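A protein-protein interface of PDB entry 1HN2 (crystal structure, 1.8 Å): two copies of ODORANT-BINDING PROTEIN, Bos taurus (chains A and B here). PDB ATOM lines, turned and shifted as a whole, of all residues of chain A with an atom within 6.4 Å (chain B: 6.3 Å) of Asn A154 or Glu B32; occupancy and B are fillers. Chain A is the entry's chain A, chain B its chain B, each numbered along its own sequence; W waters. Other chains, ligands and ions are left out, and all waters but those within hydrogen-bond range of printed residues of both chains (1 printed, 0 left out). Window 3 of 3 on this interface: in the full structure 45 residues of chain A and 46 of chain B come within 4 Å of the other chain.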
ATOM      1  N   ASN A 152      11.372  -1.566 -11.592  1.00  0.00           N
ATOM      2  CA  ASN A 152      11.244  -1.422 -10.147  1.00  0.00           C
ATOM      3  C   ASN A 152      10.922   0.018  -9.764  1.00  0.00           C
ATOM      4  O   ASN A 152      11.598   0.953 -10.194  1.00  0.00           O
ATOM      5  CB  ASN A 152      12.536  -1.863  -9.450  1.00  0.00           C
ATOM      6  CG  ASN A 152      12.329  -2.155  -7.976  1.00  0.00           C
ATOM      7  OD1 ASN A 152      11.614  -3.090  -7.613  1.00  0.00           O
ATOM      8  ND2 ASN A 152      12.949  -1.352  -7.117  1.00  0.00           N
ATOM      9  N   GLU A 153       9.882   0.187  -8.953  1.00  0.00           N
ATOM     10  CA  GLU A 153       9.453   1.509  -8.506  1.00  0.00           C
ATOM     11  C   GLU A 153      10.540   2.244  -7.729  1.00  0.00           C
ATOM     12  O   GLU A 153      10.787   3.430  -7.952  1.00  0.00           O
ATOM     13  CB  GLU A 153       8.204   1.386  -7.624  1.00  0.00           C
ATOM     14  CG  GLU A 153       8.361   0.441  -6.444  1.00  0.00           C
ATOM     15  CD  GLU A 153       7.150   0.439  -5.527  1.00  0.00           C
ATOM     16  OE1 GLU A 153       6.028   0.668  -6.025  1.00  0.00           O
ATOM     17  OE2 GLU A 153       7.315   0.193  -4.312  1.00  0.00           O
ATOM     18  N   ASN A 154      11.182   1.527  -6.815  1.00  0.00           N
ATOM     19  CA  ASN A 154      12.229   2.092  -5.975  1.00  0.00           C
ATOM     20  C   ASN A 154      13.539   2.271  -6.743  1.00  0.00           C
ATOM     21  O   ASN A 154      14.377   1.369  -6.764  1.00  0.00           O
ATOM     22  CB  ASN A 154      12.449   1.178  -4.766  1.00  0.00           C
ATOM     23  CG  ASN A 154      13.268   1.835  -3.674  1.00  0.00           C
ATOM     24  OD1 ASN A 154      13.702   1.175  -2.728  1.00  0.00           O
ATOM     25  ND2 ASN A 154      13.476   3.142  -3.791  1.00  0.00           N
ATOM     26  N   HIS A 155      13.715   3.437  -7.363  1.00  0.00           N
ATOM     27  CA  HIS A 155      14.925   3.730  -8.133  1.00  0.00           C
ATOM     28  C   HIS A 155      15.440   5.159  -7.909  1.00  0.00           C
ATOM     29  O   HIS A 155      14.698   6.036  -7.465  1.00  0.00           O
ATOM     30  CB  HIS A 155      14.661   3.498  -9.624  1.00  0.00           C
ATOM     31  CG  HIS A 155      13.547   4.329 -10.180  1.00  0.00           C
ATOM     32  ND1 HIS A 155      13.641   5.695 -10.336  1.00  0.00           N
ATOM     33  CD2 HIS A 155      12.309   3.986 -10.609  1.00  0.00           C
ATOM     34  CE1 HIS A 155      12.510   6.158 -10.837  1.00  0.00           C
ATOM     35  NE2 HIS A 155      11.685   5.142 -11.012  1.00  0.00           N
ATOM     36  N   PRO A 156      16.729   5.405  -8.215  1.00  0.00           N
ATOM     37  CA  PRO A 156      17.357   6.722  -8.048  1.00  0.00           C
ATOM     38  C   PRO A 156      16.712   7.816  -8.897  1.00  0.00           C
ATOM     39  O   PRO A 156      16.065   7.532  -9.907  1.00  0.00           O
ATOM     40  CB  PRO A 156      18.809   6.471  -8.461  1.00  0.00           C
ATOM     41  CG  PRO A 156      19.007   5.012  -8.182  1.00  0.00           C
ATOM     42  CD  PRO A 156      17.718   4.415  -8.675  1.00  0.00           C
ATOM     43  N   GLU B  28      18.826 -10.586   2.602  1.00  0.00           N
ATOM     44  CA  GLU B  28      18.960  -9.312   3.309  1.00  0.00           C
ATOM     45  C   GLU B  28      19.933  -8.342   2.637  1.00  0.00           C
ATOM     46  O   GLU B  28      19.781  -7.123   2.746  1.00  0.00           O
ATOM     47  CB  GLU B  28      19.402  -9.552   4.765  1.00  0.00           C
ATOM     48  CG  GLU B  28      20.885  -9.779   4.941  1.00  0.00           C
ATOM     49  CD  GLU B  28      21.248 -10.318   6.316  1.00  0.00           C
ATOM     50  OE1 GLU B  28      22.458 -10.477   6.595  1.00  0.00           O
ATOM     51  OE2 GLU B  28      20.326 -10.587   7.115  1.00  0.00           O
ATOM     52  N   ILE B  30      20.257  -7.722  -0.490  1.00  0.00           N
ATOM     53  CA  ILE B  30      19.682  -7.031  -1.637  1.00  0.00           C
ATOM     54  C   ILE B  30      18.264  -6.504  -1.441  1.00  0.00           C
ATOM     55  O   ILE B  30      17.636  -6.046  -2.395  1.00  0.00           O
ATOM     56  CB  ILE B  30      19.721  -7.907  -2.907  1.00  0.00           C
ATOM     57  CG1 ILE B  30      18.988  -9.226  -2.666  1.00  0.00           C
ATOM     58  CG2 ILE B  30      21.173  -8.153  -3.314  1.00  0.00           C
ATOM     59  CD1 ILE B  30      18.895 -10.114  -3.925  1.00  0.00           C
ATOM     60  N   GLN B  31      17.773  -6.571  -0.206  1.00  0.00           N
ATOM     61  CA  GLN B  31      16.449  -6.057   0.135  1.00  0.00           C
ATOM     62  C   GLN B  31      16.582  -4.548   0.225  1.00  0.00           C
ATOM     63  O   GLN B  31      17.692  -4.021   0.190  1.00  0.00           O
ATOM     64  CB  GLN B  31      15.996  -6.591   1.498  1.00  0.00           C
ATOM     65  CG  GLN B  31      15.272  -7.905   1.475  1.00  0.00           C
ATOM     66  CD  GLN B  31      15.026  -8.443   2.874  1.00  0.00           C
ATOM     67  OE1 GLN B  31      14.883  -7.677   3.829  1.00  0.00           O
ATOM     68  NE2 GLN B  31      14.964  -9.765   3.002  1.00  0.00           N
ATOM     69  N   GLU B  32      15.457  -3.848   0.352  1.00  0.00           N
ATOM     70  CA  GLU B  32      15.500  -2.396   0.459  1.00  0.00           C
ATOM     71  C   GLU B  32      16.477  -2.064   1.580  1.00  0.00           C
ATOM     72  O   GLU B  32      16.472  -2.710   2.627  1.00  0.00           O
ATOM     73  CB  GLU B  32      14.104  -1.835   0.760  1.00  0.00           C
ATOM     74  CG  GLU B  32      14.032  -0.323   0.748  1.00  0.00           C
ATOM     75  CD  GLU B  32      12.606   0.196   0.631  1.00  0.00           C
ATOM     76  OE1 GLU B  32      11.973  -0.036  -0.424  1.00  0.00           O
ATOM     77  OE2 GLU B  32      12.123   0.833   1.591  1.00  0.00           O
ATOM     78  N   ASN B  33      17.324  -1.067   1.335  1.00  0.00           N
ATOM     79  CA  ASN B  33      18.357  -0.635   2.273  1.00  0.00           C
ATOM     80  C   ASN B  33      19.509  -1.633   2.404  1.00  0.00           C
ATOM     81  O   ASN B  33      20.368  -1.492   3.275  1.00  0.00           O
ATOM     82  CB  ASN B  33      17.749  -0.331   3.643  1.00  0.00           C
ATOM     83  CG  ASN B  33      17.026   1.000   3.664  1.00  0.00           C
ATOM     84  OD1 ASN B  33      17.626   2.045   3.405  1.00  0.00           O
ATOM     85  ND2 ASN B  33      15.733   0.972   3.963  1.00  0.00           N
ATOM     86  N   GLY B  34      19.524  -2.639   1.535  1.00  0.00           N
ATOM     87  CA  GLY B  34      20.597  -3.619   1.559  1.00  0.00           C
ATOM     88  C   GLY B  34      21.778  -3.037   0.799  1.00  0.00           C
ATOM     89  O   GLY B  34      21.573  -2.355  -0.202  1.00  0.00           O
ATOM     90  N   ARG B  37      21.949  -3.770  -3.280  1.00  0.00           N
ATOM     91  CA  ARG B  37      20.820  -3.467  -4.171  1.00  0.00           C
ATOM     92  C   ARG B  37      21.346  -2.257  -4.946  1.00  0.00           C
ATOM     93  O   ARG B  37      20.865  -1.129  -4.817  1.00  0.00           O
ATOM     94  CB  ARG B  37      19.574  -3.085  -3.363  1.00  0.00           C
ATOM     95  CG  ARG B  37      18.390  -2.664  -4.224  1.00  0.00           C
ATOM     96  CD  ARG B  37      17.167  -2.355  -3.382  1.00  0.00           C
ATOM     97  NE  ARG B  37      16.508  -3.581  -2.966  1.00  0.00           N
ATOM     98  CZ  ARG B  37      15.307  -3.968  -3.384  1.00  0.00           C
ATOM     99  NH1 ARG B  37      14.613  -3.219  -4.231  1.00  0.00           N
ATOM    100  NH2 ARG B  37      14.810  -5.120  -2.967  1.00  0.00           N
ATOM    101  N   TYR B  39      22.257   0.077  -8.175  1.00  0.00           N
ATOM    102  CA  TYR B  39      21.859   0.522  -9.507  1.00  0.00           C
ATOM    103  C   TYR B  39      23.108   1.079 -10.190  1.00  0.00           C
ATOM    104  O   TYR B  39      23.587   2.144  -9.814  1.00  0.00           O
ATOM    105  CB  TYR B  39      20.804   1.628  -9.420  1.00  0.00           C
ATOM    106  CG  TYR B  39      19.402   1.124  -9.164  1.00  0.00           C
ATOM    107  CD1 TYR B  39      18.974   0.810  -7.876  1.00  0.00           C
ATOM    108  CD2 TYR B  39      18.506   0.949 -10.221  1.00  0.00           C
ATOM    109  CE1 TYR B  39      17.680   0.333  -7.643  1.00  0.00           C
ATOM    110  CE2 TYR B  39      17.215   0.474 -10.000  1.00  0.00           C
ATOM    111  CZ  TYR B  39      16.810   0.169  -8.713  1.00  0.00           C
ATOM    112  OH  TYR B  39      15.534  -0.302  -8.496  1.00  0.00           O
ATOM    113  N   LYS B  59      20.469   2.839  -1.949  1.00  0.00           N
ATOM    114  CA  LYS B  59      19.825   3.618  -0.902  1.00  0.00           C
ATOM    115  C   LYS B  59      20.088   3.039   0.486  1.00  0.00           C
ATOM    116  O   LYS B  59      20.080   1.822   0.732  1.00  0.00           O
ATOM    117  CB  LYS B  59      18.351   3.853  -1.274  1.00  0.00           C
ATOM    118  CG  LYS B  59      17.281   3.854  -0.291  1.00  0.00           C
ATOM    119  CD  LYS B  59      16.093   3.788  -0.976  1.00  0.00           C
ATOM    120  CE  LYS B  59      14.863   3.786  -0.099  1.00  0.00           C
ATOM    121  NZ  LYS B  59      15.176   3.476   1.404  1.00  0.00           N
ATOM    122  N   TRP B  64      19.282   7.915  -1.144  1.00  0.00           N
ATOM    123  CA  TRP B  64      20.134   7.439  -2.207  1.00  0.00           C
ATOM    124  C   TRP B  64      21.531   8.002  -2.092  1.00  0.00           C
ATOM    125  O   TRP B  64      21.712   9.196  -1.862  1.00  0.00           O
ATOM    126  CB  TRP B  64      19.530   7.808  -3.559  1.00  0.00           C
ATOM    127  CG  TRP B  64      18.338   6.984  -3.921  1.00  0.00           C
ATOM    128  CD1 TRP B  64      17.024   7.348  -3.832  1.00  0.00           C
ATOM    129  CD2 TRP B  64      18.353   5.643  -4.413  1.00  0.00           C
ATOM    130  NE1 TRP B  64      16.219   6.311  -4.241  1.00  0.00           N
ATOM    131  CE2 TRP B  64      17.009   5.251  -4.601  1.00  0.00           C
ATOM    132  CE3 TRP B  64      19.374   4.728  -4.710  1.00  0.00           C
ATOM    133  CZ2 TRP B  64      16.658   3.981  -5.078  1.00  0.00           C
ATOM    134  CZ3 TRP B  64      19.026   3.466  -5.183  1.00  0.00           C
ATOM    135  CH2 TRP B  64      17.677   3.106  -5.361  1.00  0.00           C
HETATM  136  O   HOH W   1      14.781  -0.416  -4.985  1.00  0.00           O
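O of Gln B31 lies close to NE of Arg B37, 3.4 Å away.
NE of Arg B37 is in hydrogen-bond range of O of Ile B30 (2.8 Å).
The side-chain amide nitrogen (ND2) of Asn A152 sits at hydrogen-bond distance from the backbone carbonyl oxygen (O) of Asn A154 (3.1 Å).
The side-chain amide oxygen (OD1) of Asn B33 lies within hydrogen-bond range of the side-chain amino group (NZ) of Lys B59 (3.5 Å).
Printed residues of chain A that touch a printed residue of chain B: Asn A152, Asn A154, His A155 and Pro A156.
Hydrophobic or aromatic side chains of chain A that line the printed part of chain B: His A155 and Pro A156.
Printed residues of chain B that touch a printed residue of chain A: Glu B32, Arg B37, Tyr B39, Lys B59 and Trp B64.
Along chain B the printed residues that touch a printed residue of chain A span positions 32 to 64.
Among the printed residues, 10 pairs touch across the chains.
Among the printed residues, no Asp or Glu carboxylate lies within 4 Å of a Lys or Arg side-chain nitrogen of the other chain.
No position is printed for both chains.
Of the 10 pairs that touch across the chains among the printed residues, none has its exchanged pair printed and touching as well.
Water W1 lies within hydrogen-bond range of the backbone carbonyl oxygen of Asn A154 (2.6 Å), the guanidinium group of Arg B37 (2.9 Å) and the side-chain amide nitrogen of Asn A152 (3.0 Å).
O of Asn A154 is in hydrogen-bond range of OH of Tyr B39, at 2.7 Å.
OD1 of Asn A154 sits close to OE1 of Glu B32.
ND2 of Asn A152 is in hydrogen-bond range of OH of Tyr B39, 3.1 Å away.
Among the printed residues, merely in contact across the chains: Asn A152 with Arg B37, Asn A154 with Lys B59, Asn A154 with Trp B64, His A155 with Tyr B39, His A155 with Trp B64, Pro A156 with Tyr B39 and Pro A156 with Trp B64.
Of chain B, only Glu B32 (3.1 Å), Tyr B39 (2.7 Å), Lys B59 (3.9 Å) and Trp B64 (3.5 Å) come within 4 Å of Asn A154.
Of the printed residues of chain B, His A155 touches Tyr B39 and Trp B64.
Of the printed residues of chain A, Arg B37 touches Asn A152.
Of the printed residues of chain A, Trp B64 touches Asn A154, His A155 and Pro A156.
The nearest residue of chain A that does not touch Glu B32 is Glu A153 (6.1 Å).
The nearest printed residue of chain B that does not touch Pro A156 is Lys B59 (6.8 Å).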
